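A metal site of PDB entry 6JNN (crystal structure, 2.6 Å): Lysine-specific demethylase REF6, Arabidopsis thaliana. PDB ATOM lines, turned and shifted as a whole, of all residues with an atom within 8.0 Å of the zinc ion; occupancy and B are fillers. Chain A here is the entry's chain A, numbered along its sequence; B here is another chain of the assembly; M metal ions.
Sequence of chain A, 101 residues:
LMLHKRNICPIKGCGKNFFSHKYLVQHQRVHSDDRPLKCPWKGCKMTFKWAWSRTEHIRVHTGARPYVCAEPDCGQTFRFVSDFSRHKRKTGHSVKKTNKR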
ATOM      1  N   ILE A   8       5.847  25.005 -17.078  1.00  0.00           N
ATOM      2  CA  ILE A   8       4.421  24.708 -16.926  1.00  0.00           C
ATOM      3  C   ILE A   8       4.162  23.966 -15.628  1.00  0.00           C
ATOM      4  O   ILE A   8       4.883  22.998 -15.298  1.00  0.00           O
ATOM      5  CB  ILE A   8       3.888  23.909 -18.137  1.00  0.00           C
ATOM      6  CG1 ILE A   8       3.948  24.749 -19.428  1.00  0.00           C
ATOM      7  CG2 ILE A   8       2.462  23.442 -17.892  1.00  0.00           C
ATOM      8  CD1 ILE A   8       2.850  25.770 -19.575  1.00  0.00           C
ATOM      9  N   CYS A   9       3.127  24.414 -14.909  1.00  0.00           N
ATOM     10  CA  CYS A   9       2.726  23.781 -13.652  1.00  0.00           C
ATOM     11  C   CYS A   9       2.199  22.359 -13.917  1.00  0.00           C
ATOM     12  O   CYS A   9       1.328  22.180 -14.747  1.00  0.00           O
ATOM     13  CB  CYS A   9       1.676  24.598 -12.919  1.00  0.00           C
ATOM     14  SG  CYS A   9       1.213  23.920 -11.317  1.00  0.00           S
ATOM     15  N   PRO A  10       2.773  21.353 -13.218  1.00  0.00           N
ATOM     16  CA  PRO A  10       2.284  19.989 -13.386  1.00  0.00           C
ATOM     17  C   PRO A  10       0.920  19.725 -12.769  1.00  0.00           C
ATOM     18  O   PRO A  10       0.330  18.693 -13.119  1.00  0.00           O
ATOM     19  CB  PRO A  10       3.359  19.137 -12.754  1.00  0.00           C
ATOM     20  CG  PRO A  10       4.019  20.034 -11.781  1.00  0.00           C
ATOM     21  CD  PRO A  10       3.977  21.419 -12.382  1.00  0.00           C
ATOM     22  N   ILE A  11       0.383  20.630 -11.935  1.00  0.00           N
ATOM     23  CA  ILE A  11      -0.910  20.339 -11.289  1.00  0.00           C
ATOM     24  C   ILE A  11      -2.052  20.363 -12.266  1.00  0.00           C
ATOM     25  O   ILE A  11      -2.372  21.421 -12.814  1.00  0.00           O
ATOM     26  CB  ILE A  11      -1.171  21.259 -10.089  1.00  0.00           C
ATOM     27  CG1 ILE A  11      -0.029  21.102  -9.052  1.00  0.00           C
ATOM     28  CG2 ILE A  11      -2.570  21.077  -9.514  1.00  0.00           C
ATOM     29  CD1 ILE A  11      -0.212  20.027  -7.986  1.00  0.00           C
ATOM     30  N   LYS A  12      -2.648  19.199 -12.462  1.00  0.00           N
ATOM     31  CA  LYS A  12      -3.750  19.033 -13.398  1.00  0.00           C
ATOM     32  C   LYS A  12      -4.885  19.979 -13.004  1.00  0.00           C
ATOM     33  O   LYS A  12      -5.564  19.769 -11.991  1.00  0.00           O
ATOM     34  CB  LYS A  12      -4.199  17.581 -13.424  1.00  0.00           C
ATOM     35  N   GLY A  13      -5.137  20.972 -13.842  1.00  0.00           N
ATOM     36  CA  GLY A  13      -6.182  21.960 -13.538  1.00  0.00           C
ATOM     37  C   GLY A  13      -5.707  23.396 -13.654  1.00  0.00           C
ATOM     38  O   GLY A  13      -6.502  24.276 -14.024  1.00  0.00           O
ATOM     39  N   CYS A  14      -4.404  23.656 -13.404  1.00  0.00           N
ATOM     40  CA  CYS A  14      -3.789  24.911 -13.836  1.00  0.00           C
ATOM     41  C   CYS A  14      -2.516  24.462 -14.512  1.00  0.00           C
ATOM     42  O   CYS A  14      -1.571  24.046 -13.849  1.00  0.00           O
ATOM     43  CB  CYS A  14      -3.526  25.967 -12.709  1.00  0.00           C
ATOM     44  SG  CYS A  14      -1.983  25.918 -11.716  1.00  0.00           S
ATOM     45  N   GLY A  15      -2.549  24.429 -15.833  1.00  0.00           N
ATOM     46  CA  GLY A  15      -1.359  24.125 -16.631  1.00  0.00           C
ATOM     47  C   GLY A  15      -0.732  25.465 -16.903  1.00  0.00           C
ATOM     48  O   GLY A  15      -0.218  25.693 -18.047  1.00  0.00           O
ATOM     49  N   LYS A  16      -0.668  26.347 -15.901  1.00  0.00           N
ATOM     50  CA  LYS A  16      -0.165  27.700 -16.112  1.00  0.00           C
ATOM     51  C   LYS A  16       1.326  27.696 -16.459  1.00  0.00           C
ATOM     52  O   LYS A  16       2.060  26.738 -16.147  1.00  0.00           O
ATOM     53  CB  LYS A  16      -0.363  28.600 -14.904  1.00  0.00           C
ATOM     54  CG  LYS A  16      -1.812  28.850 -14.473  1.00  0.00           C
ATOM     55  CD  LYS A  16      -1.919  30.178 -13.703  1.00  0.00           C
ATOM     56  CE  LYS A  16      -3.174  30.997 -14.020  1.00  0.00           C
ATOM     57  NZ  LYS A  16      -2.938  32.422 -13.613  1.00  0.00           N
ATOM     58  N   ASN A  17       1.710  28.726 -17.211  1.00  0.00           N
ATOM     59  CA  ASN A  17       3.041  28.867 -17.771  1.00  0.00           C
ATOM     60  C   ASN A  17       3.755  30.043 -17.118  1.00  0.00           C
ATOM     61  O   ASN A  17       3.138  31.134 -16.955  1.00  0.00           O
ATOM     62  CB  ASN A  17       2.951  29.046 -19.305  1.00  0.00           C
ATOM     63  CG  ASN A  17       4.169  29.716 -19.895  1.00  0.00           C
ATOM     64  OD1 ASN A  17       5.226  29.101 -20.044  1.00  0.00           O
ATOM     65  ND2 ASN A  17       4.045  30.984 -20.203  1.00  0.00           N
ATOM     66  N   PHE A  18       5.038  29.873 -16.799  1.00  0.00           N
ATOM     67  CA  PHE A  18       5.778  30.859 -16.015  1.00  0.00           C
ATOM     68  C   PHE A  18       7.116  31.204 -16.613  1.00  0.00           C
ATOM     69  O   PHE A  18       7.832  30.288 -17.033  1.00  0.00           O
ATOM     70  CB  PHE A  18       6.023  30.367 -14.583  1.00  0.00           C
ATOM     71  CG  PHE A  18       4.778  29.935 -13.855  1.00  0.00           C
ATOM     72  CD1 PHE A  18       3.829  30.875 -13.469  1.00  0.00           C
ATOM     73  CD2 PHE A  18       4.561  28.579 -13.571  1.00  0.00           C
ATOM     74  CE1 PHE A  18       2.667  30.469 -12.834  1.00  0.00           C
ATOM     75  CE2 PHE A  18       3.406  28.181 -12.927  1.00  0.00           C
ATOM     76  CZ  PHE A  18       2.460  29.114 -12.549  1.00  0.00           C
ATOM     77  N   LEU A  24       8.365  28.755 -10.908  1.00  0.00           N
ATOM     78  CA  LEU A  24       7.496  27.566 -11.040  1.00  0.00           C
ATOM     79  C   LEU A  24       7.486  26.768  -9.716  1.00  0.00           C
ATOM     80  O   LEU A  24       6.452  26.287  -9.290  1.00  0.00           O
ATOM     81  CB  LEU A  24       7.860  26.690 -12.221  1.00  0.00           C
ATOM     82  CG  LEU A  24       6.869  25.562 -12.603  1.00  0.00           C
ATOM     83  CD1 LEU A  24       7.113  25.114 -14.054  1.00  0.00           C
ATOM     84  CD2 LEU A  24       6.854  24.301 -11.707  1.00  0.00           C
ATOM     85  N   HIS A  27       5.547  28.976  -7.128  1.00  0.00           N
ATOM     86  CA  HIS A  27       4.134  28.918  -7.449  1.00  0.00           C
ATOM     87  C   HIS A  27       3.393  27.826  -6.707  1.00  0.00           C
ATOM     88  O   HIS A  27       2.176  27.905  -6.535  1.00  0.00           O
ATOM     89  CB  HIS A  27       3.931  28.806  -8.969  1.00  0.00           C
ATOM     90  CG  HIS A  27       2.576  28.303  -9.376  1.00  0.00           C
ATOM     91  ND1 HIS A  27       1.456  29.096  -9.373  1.00  0.00           N
ATOM     92  CD2 HIS A  27       2.166  27.058  -9.759  1.00  0.00           C
ATOM     93  CE1 HIS A  27       0.405  28.359  -9.732  1.00  0.00           C
ATOM     94  NE2 HIS A  27       0.815  27.142 -10.023  1.00  0.00           N
ATOM     95  N   GLN A  28       4.088  26.802  -6.228  1.00  0.00           N
ATOM     96  CA  GLN A  28       3.336  25.658  -5.742  1.00  0.00           C
ATOM     97  C   GLN A  28       2.576  25.899  -4.453  1.00  0.00           C
ATOM     98  O   GLN A  28       1.590  25.252  -4.235  1.00  0.00           O
ATOM     99  CB  GLN A  28       4.191  24.440  -5.685  1.00  0.00           C
ATOM    100  CG  GLN A  28       4.937  24.113  -6.999  1.00  0.00           C
ATOM    101  CD  GLN A  28       4.017  23.878  -8.228  1.00  0.00           C
ATOM    102  OE1 GLN A  28       4.212  24.495  -9.274  1.00  0.00           O
ATOM    103  NE2 GLN A  28       2.988  23.026  -8.063  1.00  0.00           N
ATOM    104  N   ARG A  29       2.980  26.914  -3.710  1.00  0.00           N
ATOM    105  CA  ARG A  29       2.298  27.273  -2.500  1.00  0.00           C
ATOM    106  C   ARG A  29       0.814  27.521  -2.727  1.00  0.00           C
ATOM    107  O   ARG A  29      -0.022  27.182  -1.893  1.00  0.00           O
ATOM    108  CB  ARG A  29       2.978  28.435  -1.817  1.00  0.00           C
ATOM    109  CG  ARG A  29       2.918  29.742  -2.613  1.00  0.00           C
ATOM    110  CD  ARG A  29       3.796  30.810  -1.995  1.00  0.00           C
ATOM    111  NE  ARG A  29       5.188  30.662  -2.354  1.00  0.00           N
ATOM    112  CZ  ARG A  29       6.177  31.313  -1.789  1.00  0.00           C
ATOM    113  NH1 ARG A  29       5.932  32.200  -0.841  1.00  0.00           N
ATOM    114  NH2 ARG A  29       7.436  31.097  -2.211  1.00  0.00           N
ATOM    115  N   VAL A  30       0.471  28.032  -3.892  1.00  0.00           N
ATOM    116  CA  VAL A  30      -0.936  28.121  -4.380  1.00  0.00           C
ATOM    117  C   VAL A  30      -1.739  26.853  -4.100  1.00  0.00           C
ATOM    118  O   VAL A  30      -2.907  26.901  -3.765  1.00  0.00           O
ATOM    119  CB  VAL A  30      -0.960  28.452  -5.892  1.00  0.00           C
ATOM    120  CG1 VAL A  30      -2.359  28.353  -6.444  1.00  0.00           C
ATOM    121  CG2 VAL A  30      -0.365  29.835  -6.130  1.00  0.00           C
ATOM    122  N   HIS A  31      -1.128  25.710  -4.246  1.00  0.00           N
ATOM    123  CA  HIS A  31      -1.862  24.457  -4.148  1.00  0.00           C
ATOM    124  C   HIS A  31      -1.845  23.865  -2.737  1.00  0.00           C
ATOM    125  O   HIS A  31      -2.622  22.997  -2.470  1.00  0.00           O
ATOM    126  CB  HIS A  31      -1.388  23.469  -5.213  1.00  0.00           C
ATOM    127  CG  HIS A  31      -1.438  23.998  -6.619  1.00  0.00           C
ATOM    128  ND1 HIS A  31      -2.602  24.364  -7.276  1.00  0.00           N
ATOM    129  CD2 HIS A  31      -0.442  24.214  -7.504  1.00  0.00           C
ATOM    130  CE1 HIS A  31      -2.306  24.812  -8.471  1.00  0.00           C
ATOM    131  NE2 HIS A  31      -1.011  24.710  -8.655  1.00  0.00           N
ATOM    132  P    DG B   7       0.447  32.746 -10.211  1.00  0.00           P
ATOM    133  OP1  DG B   7      -0.786  32.066 -10.579  1.00  0.00           O
ATOM    134  OP2  DG B   7       1.380  31.987  -9.364  1.00  0.00           O
ATOM    135  O5'  DG B   7       1.263  33.343 -11.464  1.00  0.00           O
ATOM    136  C5'  DG B   7       0.554  34.217 -12.346  1.00  0.00           C
ATOM    137  C4'  DG B   7       1.442  35.248 -12.993  1.00  0.00           C
ATOM    138  O4'  DG B   7       1.589  36.409 -12.126  1.00  0.00           O
ATOM    139  C3'  DG B   7       2.860  34.827 -13.393  1.00  0.00           C
ATOM    140  O3'  DG B   7       3.155  35.569 -14.598  1.00  0.00           O
ATOM    141  C2'  DG B   7       3.676  35.373 -12.246  1.00  0.00           C
ATOM    142  C1'  DG B   7       2.964  36.685 -11.950  1.00  0.00           C
ATOM    143  N9   DG B   7       3.127  37.180 -10.584  1.00  0.00           N
ATOM    144  C8   DG B   7       3.079  36.430  -9.449  1.00  0.00           C
ATOM    145  N7   DG B   7       3.268  37.133  -8.363  1.00  0.00           N
ATOM    146  C5   DG B   7       3.399  38.435  -8.815  1.00  0.00           C
ATOM    147  C6   DG B   7       3.607  39.644  -8.107  1.00  0.00           C
ATOM    148  O6   DG B   7       3.698  39.807  -6.881  1.00  0.00           O
ATOM    149  N1   DG B   7       3.669  40.744  -8.960  1.00  0.00           N
ATOM    150  C2   DG B   7       3.554  40.687 -10.325  1.00  0.00           C
ATOM    151  N2   DG B   7       3.656  41.846 -10.972  1.00  0.00           N
ATOM    152  N3   DG B   7       3.382  39.561 -11.013  1.00  0.00           N
ATOM    153  C4   DG B   7       3.312  38.483 -10.195  1.00  0.00           C
HETATM  154 ZN    ZN M   1      -0.142  25.409 -10.753  1.00  0.00          ZN
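O of Lys 16 lies within hydrogen-bond range of N of Cys 9, at 2.8 Å. OP2 of DG 7 of chain B lies within hydrogen-bond range of a ring nitrogen (ND1) of His 27. SG of Cys 9 lies close to N of Ile 11 (3.4 Å). The side-chain sulfur (SG) of Cys 9 lies close to the side-chain amide oxygen (OE1) of Gln 28, at 3.7 Å.
The nearest printed residue that does not touch the zinc ion is Ile 11 (4.3 Å).
The zinc ion is bound by SG of Cys 9 (2.1 Å), NE2 of His 27 (2.1 Å), SG of Cys 14 (2.1 Å) and NE2 of His 31 (2.4 Å).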
